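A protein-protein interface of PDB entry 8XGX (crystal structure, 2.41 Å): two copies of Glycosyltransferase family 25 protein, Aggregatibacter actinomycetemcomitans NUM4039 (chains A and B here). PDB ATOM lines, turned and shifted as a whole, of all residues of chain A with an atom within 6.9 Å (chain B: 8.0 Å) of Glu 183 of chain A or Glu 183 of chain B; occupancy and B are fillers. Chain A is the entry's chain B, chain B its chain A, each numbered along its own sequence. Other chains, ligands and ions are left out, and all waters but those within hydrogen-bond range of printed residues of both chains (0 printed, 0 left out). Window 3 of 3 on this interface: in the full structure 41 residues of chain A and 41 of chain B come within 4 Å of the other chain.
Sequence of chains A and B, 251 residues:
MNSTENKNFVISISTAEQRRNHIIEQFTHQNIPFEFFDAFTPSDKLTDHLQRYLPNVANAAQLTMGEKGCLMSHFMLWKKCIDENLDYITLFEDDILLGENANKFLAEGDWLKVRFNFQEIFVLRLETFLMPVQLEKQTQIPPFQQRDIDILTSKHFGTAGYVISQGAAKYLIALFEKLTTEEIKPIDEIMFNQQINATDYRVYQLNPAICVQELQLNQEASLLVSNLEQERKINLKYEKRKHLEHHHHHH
The side-chain carboxylate (OE1) of Glu 182 of chain B lies within salt-bridge range of the side-chain amino group (NZ) of Lys 178 of chain A (3.0 Å).
The side-chain amino group (NZ) of Lys 185 of chain A lies within hydrogen-bond range of the backbone carbonyl oxygen (O) of Gln 194 of chain B (3.2 Å).
OE2 of Glu 183 of chain A sits close to OE2 of Glu 183 of chain B (2.9 Å).
The backbone carbonyl oxygen of Gln 194 of chain A sits close to the side-chain amino group of Lys 185 of chain B (2.3 Å).
Of chain B, only Glu 183 (2.9 Å) comes within 4 Å of Glu 183 of chain A.
Glu 183 of chain B touches just one residue of chain A: Glu 183.
No residue of chain B comes within 4 Å of Thr 180 of chain A.
Of the printed residues of chain A, Gln 194 of chain B touches Lys 185 (3.2 Å) and Gln 194 (3.8 Å).
Of the printed residues of chain B, Lys 185 of chain A touches Gln 194.
Printed residues of chain A within 4 Å of Lys 185 of chain B: Gln 194.
Among the printed residues, pairs that only touch across the chains: Gln 194 of chain A with Gln 194 of chain B.
Of the 11 printed residues of chain A, 4 touch a printed residue of chain B.
Printed residues of chain A that touch a printed residue of chain B: Lys 178, Glu 183, Lys 185 and Gln 194.
Of the 16 printed residues of chain B, 4 touch a printed residue of chain A.
Among the printed residues, Asp or Glu carboxylates within 4 Å of a Lys or Arg side-chain nitrogen of the other chain: Lys 178 of chain A with Glu 182 of chain B.
Lys 178 of chain A touches Glu 182 of chain B, but with the chains exchanged Glu 182 of chain A does not touch Lys 178 of chain B (7.0 Å).
Glu 183 of chain A touches its own counterpart, Glu 183 of chain B.
Lys 185 of chain A touches Gln 194 of chain B, and with the chains exchanged Gln 194 of chain A touches Lys 185 of chain B.
Gln 194 of chain B touches its own counterpart, Gln 194 of chain A.
Of the 5 pairs that touch across the chains among the printed residues, 4 have their exchanged pair printed and touching as well.
OE1 of Glu 183 of chain B sits at hydrogen-bond distance from N of Thr 180 of chain B, 2.9 Å away.
The side-chain carboxylate of Glu 183 of chain A is in hydrogen-bond range of the backbone NH of Thr 180 of chain A (2.9 Å).
The side-chain amino group (NZ) of Lys 185 of chain A is in hydrogen-bond range of the side-chain amide oxygen (OE1) of Gln 194 of chain A (3.1 Å).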
ATOM      1  N   GLN A  62      -3.155  -5.280  30.803  1.00  0.00           N
ATOM      2  CA  GLN A  62      -3.547  -5.371  29.367  1.00  0.00           C
ATOM      3  C   GLN A  62      -3.262  -4.062  28.606  1.00  0.00           C
ATOM      4  O   GLN A  62      -3.484  -4.055  27.378  1.00  0.00           O
ATOM      5  CB  GLN A  62      -5.015  -5.795  29.235  1.00  0.00           C
ATOM      6  CG  GLN A  62      -6.032  -4.726  29.613  1.00  0.00           C
ATOM      7  CD  GLN A  62      -6.380  -4.704  31.081  1.00  0.00           C
ATOM      8  OE1 GLN A  62      -5.568  -5.006  31.950  1.00  0.00           O
ATOM      9  NE2 GLN A  62      -7.607  -4.320  31.369  1.00  0.00           N
ATOM     10  N   LYS A 178     -14.361   5.346  36.828  1.00  0.00           N
ATOM     11  CA  LYS A 178     -15.394   4.333  37.185  1.00  0.00           C
ATOM     12  C   LYS A 178     -14.918   2.917  36.835  1.00  0.00           C
ATOM     13  O   LYS A 178     -15.118   2.012  37.655  1.00  0.00           O
ATOM     14  CB  LYS A 178     -16.700   4.685  36.462  1.00  0.00           C
ATOM     15  CG  LYS A 178     -17.601   3.529  36.056  1.00  0.00           C
ATOM     16  CD  LYS A 178     -18.627   3.948  35.020  1.00  0.00           C
ATOM     17  CE  LYS A 178     -19.683   2.888  34.789  1.00  0.00           C
ATOM     18  NZ  LYS A 178     -20.836   3.420  34.022  1.00  0.00           N
ATOM     19  N   LEU A 179     -14.345   2.721  35.643  1.00  0.00           N
ATOM     20  CA  LEU A 179     -14.079   1.376  35.065  1.00  0.00           C
ATOM     21  C   LEU A 179     -13.155   0.590  35.996  1.00  0.00           C
ATOM     22  O   LEU A 179     -12.168   1.179  36.483  1.00  0.00           O
ATOM     23  CB  LEU A 179     -13.441   1.518  33.681  1.00  0.00           C
ATOM     24  CG  LEU A 179     -14.327   2.105  32.585  1.00  0.00           C
ATOM     25  CD1 LEU A 179     -13.491   2.441  31.364  1.00  0.00           C
ATOM     26  CD2 LEU A 179     -15.461   1.156  32.220  1.00  0.00           C
ATOM     27  N   THR A 180     -13.465  -0.693  36.211  1.00  0.00           N
ATOM     28  CA  THR A 180     -12.607  -1.660  36.943  1.00  0.00           C
ATOM     29  C   THR A 180     -11.367  -1.946  36.095  1.00  0.00           C
ATOM     30  O   THR A 180     -11.450  -1.780  34.856  1.00  0.00           O
ATOM     31  CB  THR A 180     -13.344  -2.976  37.240  1.00  0.00           C
ATOM     32  OG1 THR A 180     -13.709  -3.553  35.985  1.00  0.00           O
ATOM     33  CG2 THR A 180     -14.575  -2.799  38.106  1.00  0.00           C
ATOM     34  N   THR A 181     -10.285  -2.389  36.739  1.00  0.00           N
ATOM     35  CA  THR A 181      -9.034  -2.852  36.081  1.00  0.00           C
ATOM     36  C   THR A 181      -9.367  -3.765  34.890  1.00  0.00           C
ATOM     37  O   THR A 181      -8.759  -3.572  33.829  1.00  0.00           O
ATOM     38  CB  THR A 181      -8.110  -3.540  37.092  1.00  0.00           C
ATOM     39  OG1 THR A 181      -7.699  -2.555  38.045  1.00  0.00           O
ATOM     40  CG2 THR A 181      -6.900  -4.168  36.435  1.00  0.00           C
ATOM     41  N   GLU A 182     -10.309  -4.699  35.057  1.00  0.00           N
ATOM     42  CA  GLU A 182     -10.718  -5.697  34.033  1.00  0.00           C
ATOM     43  C   GLU A 182     -11.349  -4.986  32.826  1.00  0.00           C
ATOM     44  O   GLU A 182     -11.158  -5.470  31.701  1.00  0.00           O
ATOM     45  CB  GLU A 182     -11.714  -6.701  34.631  1.00  0.00           C
ATOM     46  CG  GLU A 182     -11.124  -7.668  35.651  1.00  0.00           C
ATOM     47  CD  GLU A 182     -10.533  -7.104  36.941  1.00  0.00           C
ATOM     48  OE1 GLU A 182     -11.197  -6.273  37.618  1.00  0.00           O
ATOM     49  OE2 GLU A 182      -9.405  -7.514  37.279  1.00  0.00           O
ATOM     50  N   GLU A 183     -12.085  -3.891  33.053  1.00  0.00           N
ATOM     51  CA  GLU A 183     -12.871  -3.164  32.014  1.00  0.00           C
ATOM     52  C   GLU A 183     -11.976  -2.205  31.207  1.00  0.00           C
ATOM     53  O   GLU A 183     -12.399  -1.812  30.106  1.00  0.00           O
ATOM     54  CB  GLU A 183     -14.030  -2.390  32.651  1.00  0.00           C
ATOM     55  CG  GLU A 183     -15.206  -3.260  33.076  1.00  0.00           C
ATOM     56  CD  GLU A 183     -16.214  -2.587  34.003  1.00  0.00           C
ATOM     57  OE1 GLU A 183     -15.810  -1.698  34.781  1.00  0.00           O
ATOM     58  OE2 GLU A 183     -17.415  -2.935  33.930  1.00  0.00           O
ATOM     59  N   ILE A 184     -10.792  -1.846  31.714  1.00  0.00           N
ATOM     60  CA  ILE A 184      -9.871  -0.868  31.059  1.00  0.00           C
ATOM     61  C   ILE A 184      -9.414  -1.419  29.707  1.00  0.00           C
ATOM     62  O   ILE A 184      -8.968  -2.571  29.657  1.00  0.00           O
ATOM     63  CB  ILE A 184      -8.660  -0.521  31.951  1.00  0.00           C
ATOM     64  CG1 ILE A 184      -9.084   0.233  33.214  1.00  0.00           C
ATOM     65  CG2 ILE A 184      -7.621   0.261  31.162  1.00  0.00           C
ATOM     66  CD1 ILE A 184      -9.880   1.493  32.934  1.00  0.00           C
ATOM     67  N   LYS A 185      -9.502  -0.580  28.673  1.00  0.00           N
ATOM     68  CA  LYS A 185      -8.935  -0.800  27.317  1.00  0.00           C
ATOM     69  C   LYS A 185      -8.238   0.486  26.884  1.00  0.00           C
ATOM     70  O   LYS A 185      -8.360   1.504  27.557  1.00  0.00           O
ATOM     71  CB  LYS A 185     -10.056  -1.201  26.354  1.00  0.00           C
ATOM     72  CG  LYS A 185     -10.921  -2.350  26.848  1.00  0.00           C
ATOM     73  CD  LYS A 185     -11.963  -2.791  25.840  1.00  0.00           C
ATOM     74  CE  LYS A 185     -12.496  -4.184  26.109  1.00  0.00           C
ATOM     75  NZ  LYS A 185     -13.881  -4.341  25.610  1.00  0.00           N
ATOM     76  N   ILE A 190     -12.343   2.656  23.977  1.00  0.00           N
ATOM     77  CA  ILE A 190     -13.482   3.104  24.833  1.00  0.00           C
ATOM     78  C   ILE A 190     -14.176   4.315  24.193  1.00  0.00           C
ATOM     79  O   ILE A 190     -15.393   4.245  23.994  1.00  0.00           O
ATOM     80  CB  ILE A 190     -13.015   3.357  26.276  1.00  0.00           C
ATOM     81  CG1 ILE A 190     -12.711   2.025  26.967  1.00  0.00           C
ATOM     82  CG2 ILE A 190     -14.043   4.163  27.057  1.00  0.00           C
ATOM     83  CD1 ILE A 190     -11.751   2.154  28.099  1.00  0.00           C
ATOM     84  N   GLN A 194     -16.471   1.149  22.265  1.00  0.00           N
ATOM     85  CA  GLN A 194     -17.308   0.593  23.357  1.00  0.00           C
ATOM     86  C   GLN A 194     -18.406   1.589  23.771  1.00  0.00           C
ATOM     87  O   GLN A 194     -19.517   1.125  24.050  1.00  0.00           O
ATOM     88  CB  GLN A 194     -16.415   0.185  24.528  1.00  0.00           C
ATOM     89  CG  GLN A 194     -17.183  -0.126  25.802  1.00  0.00           C
ATOM     90  CD  GLN A 194     -16.339  -0.924  26.764  1.00  0.00           C
ATOM     91  OE1 GLN A 194     -15.676  -1.893  26.385  1.00  0.00           O
ATOM     92  NE2 GLN A 194     -16.356  -0.515  28.024  1.00  0.00           N
ATOM     93  N   ASN B  56     -31.286  -8.600  32.995  1.00  0.00           N
ATOM     94  CA  ASN B  56     -30.459  -7.424  32.597  1.00  0.00           C
ATOM     95  C   ASN B  56     -30.842  -6.971  31.178  1.00  0.00           C
ATOM     96  O   ASN B  56     -30.867  -5.749  30.939  1.00  0.00           O
ATOM     97  CB  ASN B  56     -28.958  -7.720  32.728  1.00  0.00           C
ATOM     98  CG  ASN B  56     -28.523  -9.034  32.094  1.00  0.00           C
ATOM     99  OD1 ASN B  56     -29.257 -10.021  32.100  1.00  0.00           O
ATOM    100  ND2 ASN B  56     -27.313  -9.070  31.558  1.00  0.00           N
ATOM    101  N   ALA B  60     -33.232  -3.492  29.237  1.00  0.00           N
ATOM    102  CA  ALA B  60     -32.369  -2.705  28.327  1.00  0.00           C
ATOM    103  C   ALA B  60     -33.222  -2.027  27.248  1.00  0.00           C
ATOM    104  O   ALA B  60     -33.612  -2.694  26.269  1.00  0.00           O
ATOM    105  CB  ALA B  60     -31.309  -3.596  27.732  1.00  0.00           C
ATOM    106  N   GLN B  62     -32.253   0.122  25.108  1.00  0.00           N
ATOM    107  CA  GLN B  62     -31.426   0.399  23.897  1.00  0.00           C
ATOM    108  C   GLN B  62     -31.472  -0.776  22.901  1.00  0.00           C
ATOM    109  O   GLN B  62     -30.862  -0.632  21.822  1.00  0.00           O
ATOM    110  CB  GLN B  62     -29.987   0.760  24.288  1.00  0.00           C
ATOM    111  CG  GLN B  62     -29.147  -0.401  24.807  1.00  0.00           C
ATOM    112  CD  GLN B  62     -29.274  -0.623  26.297  1.00  0.00           C
ATOM    113  OE1 GLN B  62     -30.330  -0.412  26.900  1.00  0.00           O
ATOM    114  NE2 GLN B  62     -28.190  -1.077  26.904  1.00  0.00           N
ATOM    115  N   LEU B 175     -20.983 -14.261  29.929  1.00  0.00           N
ATOM    116  CA  LEU B 175     -20.791 -12.835  29.549  1.00  0.00           C
ATOM    117  C   LEU B 175     -22.152 -12.132  29.513  1.00  0.00           C
ATOM    118  O   LEU B 175     -22.291 -11.093  30.168  1.00  0.00           O
ATOM    119  CB  LEU B 175     -20.082 -12.735  28.192  1.00  0.00           C
ATOM    120  CG  LEU B 175     -19.882 -11.311  27.676  1.00  0.00           C
ATOM    121  CD1 LEU B 175     -19.049 -10.495  28.652  1.00  0.00           C
ATOM    122  CD2 LEU B 175     -19.243 -11.302  26.305  1.00  0.00           C
ATOM    123  N   PHE B 176     -23.125 -12.670  28.777  1.00  0.00           N
ATOM    124  CA  PHE B 176     -24.430 -11.994  28.571  1.00  0.00           C
ATOM    125  C   PHE B 176     -25.200 -11.974  29.898  1.00  0.00           C
ATOM    126  O   PHE B 176     -25.962 -11.019  30.109  1.00  0.00           O
ATOM    127  CB  PHE B 176     -25.185 -12.612  27.392  1.00  0.00           C
ATOM    128  CG  PHE B 176     -24.760 -12.053  26.056  1.00  0.00           C
ATOM    129  CD1 PHE B 176     -25.268 -10.848  25.596  1.00  0.00           C
ATOM    130  CD2 PHE B 176     -23.846 -12.724  25.258  1.00  0.00           C
ATOM    131  CE1 PHE B 176     -24.882 -10.335  24.367  1.00  0.00           C
ATOM    132  CE2 PHE B 176     -23.445 -12.199  24.036  1.00  0.00           C
ATOM    133  CZ  PHE B 176     -23.966 -11.009  23.591  1.00  0.00           C
ATOM    134  N   LYS B 178     -23.647 -11.761  32.843  1.00  0.00           N
ATOM    135  CA  LYS B 178     -22.799 -10.859  33.676  1.00  0.00           C
ATOM    136  C   LYS B 178     -23.140  -9.380  33.413  1.00  0.00           C
ATOM    137  O   LYS B 178     -23.233  -8.614  34.393  1.00  0.00           O
ATOM    138  CB  LYS B 178     -21.322 -11.155  33.380  1.00  0.00           C
ATOM    139  CG  LYS B 178     -20.359  -9.989  33.561  1.00  0.00           C
ATOM    140  CD  LYS B 178     -19.127 -10.032  32.679  1.00  0.00           C
ATOM    141  CE  LYS B 178     -17.919 -10.652  33.345  1.00  0.00           C
ATOM    142  NZ  LYS B 178     -16.838 -10.901  32.364  1.00  0.00           N
ATOM    143  N   LEU B 179     -23.263  -8.983  32.141  1.00  0.00           N
ATOM    144  CA  LEU B 179     -23.338  -7.566  31.692  1.00  0.00           C
ATOM    145  C   LEU B 179     -24.492  -6.850  32.400  1.00  0.00           C
ATOM    146  O   LEU B 179     -25.587  -7.427  32.485  1.00  0.00           O
ATOM    147  CB  LEU B 179     -23.547  -7.507  30.173  1.00  0.00           C
ATOM    148  CG  LEU B 179     -22.389  -7.980  29.300  1.00  0.00           C
ATOM    149  CD1 LEU B 179     -22.828  -8.106  27.853  1.00  0.00           C
ATOM    150  CD2 LEU B 179     -21.191  -7.051  29.406  1.00  0.00           C
ATOM    151  N   THR B 180     -24.252  -5.619  32.857  1.00  0.00           N
ATOM    152  CA  THR B 180     -25.289  -4.695  33.389  1.00  0.00           C
ATOM    153  C   THR B 180     -26.179  -4.237  32.232  1.00  0.00           C
ATOM    154  O   THR B 180     -25.702  -4.257  31.073  1.00  0.00           O
ATOM    155  CB  THR B 180     -24.664  -3.476  34.079  1.00  0.00           C
ATOM    156  OG1 THR B 180     -23.904  -2.788  33.086  1.00  0.00           O
ATOM    157  CG2 THR B 180     -23.774  -3.823  35.255  1.00  0.00           C
ATOM    158  N   THR B 181     -27.403  -3.809  32.542  1.00  0.00           N
ATOM    159  CA  THR B 181     -28.363  -3.212  31.576  1.00  0.00           C
ATOM    160  C   THR B 181     -27.653  -2.171  30.695  1.00  0.00           C
ATOM    161  O   THR B 181     -27.893  -2.188  29.480  1.00  0.00           O
ATOM    162  CB  THR B 181     -29.576  -2.625  32.307  1.00  0.00           C
ATOM    163  OG1 THR B 181     -30.301  -3.724  32.852  1.00  0.00           O
ATOM    164  CG2 THR B 181     -30.494  -1.842  31.400  1.00  0.00           C
ATOM    165  N   GLU B 182     -26.805  -1.314  31.270  1.00  0.00           N
ATOM    166  CA  GLU B 182     -26.112  -0.222  30.526  1.00  0.00           C
ATOM    167  C   GLU B 182     -25.092  -0.818  29.542  1.00  0.00           C
ATOM    168  O   GLU B 182     -24.887  -0.200  28.487  1.00  0.00           O
ATOM    169  CB  GLU B 182     -25.460   0.798  31.470  1.00  0.00           C
ATOM    170  CG  GLU B 182     -24.356   0.230  32.356  1.00  0.00           C
ATOM    171  CD  GLU B 182     -23.954   1.082  33.553  1.00  0.00           C
ATOM    172  OE1 GLU B 182     -23.430   2.194  33.324  1.00  0.00           O
ATOM    173  OE2 GLU B 182     -24.160   0.629  34.715  1.00  0.00           O
ATOM    174  N   GLU B 183     -24.493  -1.973  29.860  1.00  0.00           N
ATOM    175  CA  GLU B 183     -23.425  -2.622  29.042  1.00  0.00           C
ATOM    176  C   GLU B 183     -24.024  -3.439  27.882  1.00  0.00           C
ATOM    177  O   GLU B 183     -23.267  -3.771  26.958  1.00  0.00           O
ATOM    178  CB  GLU B 183     -22.541  -3.521  29.917  1.00  0.00           C
ATOM    179  CG  GLU B 183     -21.556  -2.760  30.799  1.00  0.00           C
ATOM    180  CD  GLU B 183     -20.954  -3.551  31.953  1.00  0.00           C
ATOM    181  OE1 GLU B 183     -21.553  -4.579  32.353  1.00  0.00           O
ATOM    182  OE2 GLU B 183     -19.900  -3.120  32.472  1.00  0.00           O
ATOM    183  N   ILE B 184     -25.321  -3.759  27.920  1.00  0.00           N
ATOM    184  CA  ILE B 184     -25.997  -4.584  26.872  1.00  0.00           C
ATOM    185  C   ILE B 184     -25.970  -3.836  25.535  1.00  0.00           C
ATOM    186  O   ILE B 184     -26.351  -2.656  25.499  1.00  0.00           O
ATOM    187  CB  ILE B 184     -27.443  -4.959  27.260  1.00  0.00           C
ATOM    188  CG1 ILE B 184     -27.485  -5.878  28.483  1.00  0.00           C
ATOM    189  CG2 ILE B 184     -28.181  -5.564  26.073  1.00  0.00           C
ATOM    190  CD1 ILE B 184     -26.668  -7.131  28.330  1.00  0.00           C
ATOM    191  N   LYS B 185     -25.574  -4.540  24.474  1.00  0.00           N
ATOM    192  CA  LYS B 185     -25.695  -4.109  23.056  1.00  0.00           C
ATOM    193  C   LYS B 185     -26.239  -5.286  22.250  1.00  0.00           C
ATOM    194  O   LYS B 185     -26.328  -6.397  22.767  1.00  0.00           O
ATOM    195  CB  LYS B 185     -24.333  -3.633  22.545  1.00  0.00           C
ATOM    196  CG  LYS B 185     -23.558  -2.751  23.513  1.00  0.00           C
ATOM    197  CD  LYS B 185     -22.416  -2.003  22.866  1.00  0.00           C
ATOM    198  CE  LYS B 185     -21.763  -1.020  23.816  1.00  0.00           C
ATOM    199  NZ  LYS B 185     -21.346   0.210  23.104  1.00  0.00           N
ATOM    200  N   PRO B 186     -26.674  -5.081  20.985  1.00  0.00           N
ATOM    201  CA  PRO B 186     -27.079  -6.193  20.129  1.00  0.00           C
ATOM    202  C   PRO B 186     -25.983  -7.263  20.050  1.00  0.00           C
ATOM    203  O   PRO B 186     -24.803  -6.922  20.109  1.00  0.00           O
ATOM    204  CB  PRO B 186     -27.327  -5.530  18.773  1.00  0.00           C
ATOM    205  CG  PRO B 186     -27.723  -4.110  19.136  1.00  0.00           C
ATOM    206  CD  PRO B 186     -26.856  -3.776  20.331  1.00  0.00           C
ATOM    207  N   ILE B 190     -21.428  -7.179  20.416  1.00  0.00           N
ATOM    208  CA  ILE B 190     -20.612  -7.792  21.502  1.00  0.00           C
ATOM    209  C   ILE B 190     -19.745  -8.917  20.916  1.00  0.00           C
ATOM    210  O   ILE B 190     -18.518  -8.898  21.132  1.00  0.00           O
ATOM    211  CB  ILE B 190     -21.513  -8.237  22.664  1.00  0.00           C
ATOM    212  CG1 ILE B 190     -22.037  -7.004  23.408  1.00  0.00           C
ATOM    213  CG2 ILE B 190     -20.776  -9.196  23.591  1.00  0.00           C
ATOM    214  CD1 ILE B 190     -23.255  -7.256  24.233  1.00  0.00           C
ATOM    215  N   GLN B 194     -16.988  -5.659  20.364  1.00  0.00           N
ATOM    216  CA  GLN B 194     -16.546  -5.255  21.720  1.00  0.00           C
ATOM    217  C   GLN B 194     -15.640  -6.332  22.341  1.00  0.00           C
ATOM    218  O   GLN B 194     -14.660  -5.935  22.997  1.00  0.00           O
ATOM    219  CB  GLN B 194     -17.773  -4.931  22.572  1.00  0.00           C
ATOM    220  CG  GLN B 194     -17.477  -4.853  24.060  1.00  0.00           C
ATOM    221  CD  GLN B 194     -18.620  -4.232  24.817  1.00  0.00           C
ATOM    222  OE1 GLN B 194     -19.098  -3.156  24.459  1.00  0.00           O
ATOM    223  NE2 GLN B 194     -19.069  -4.913  25.863  1.00  0.00           N
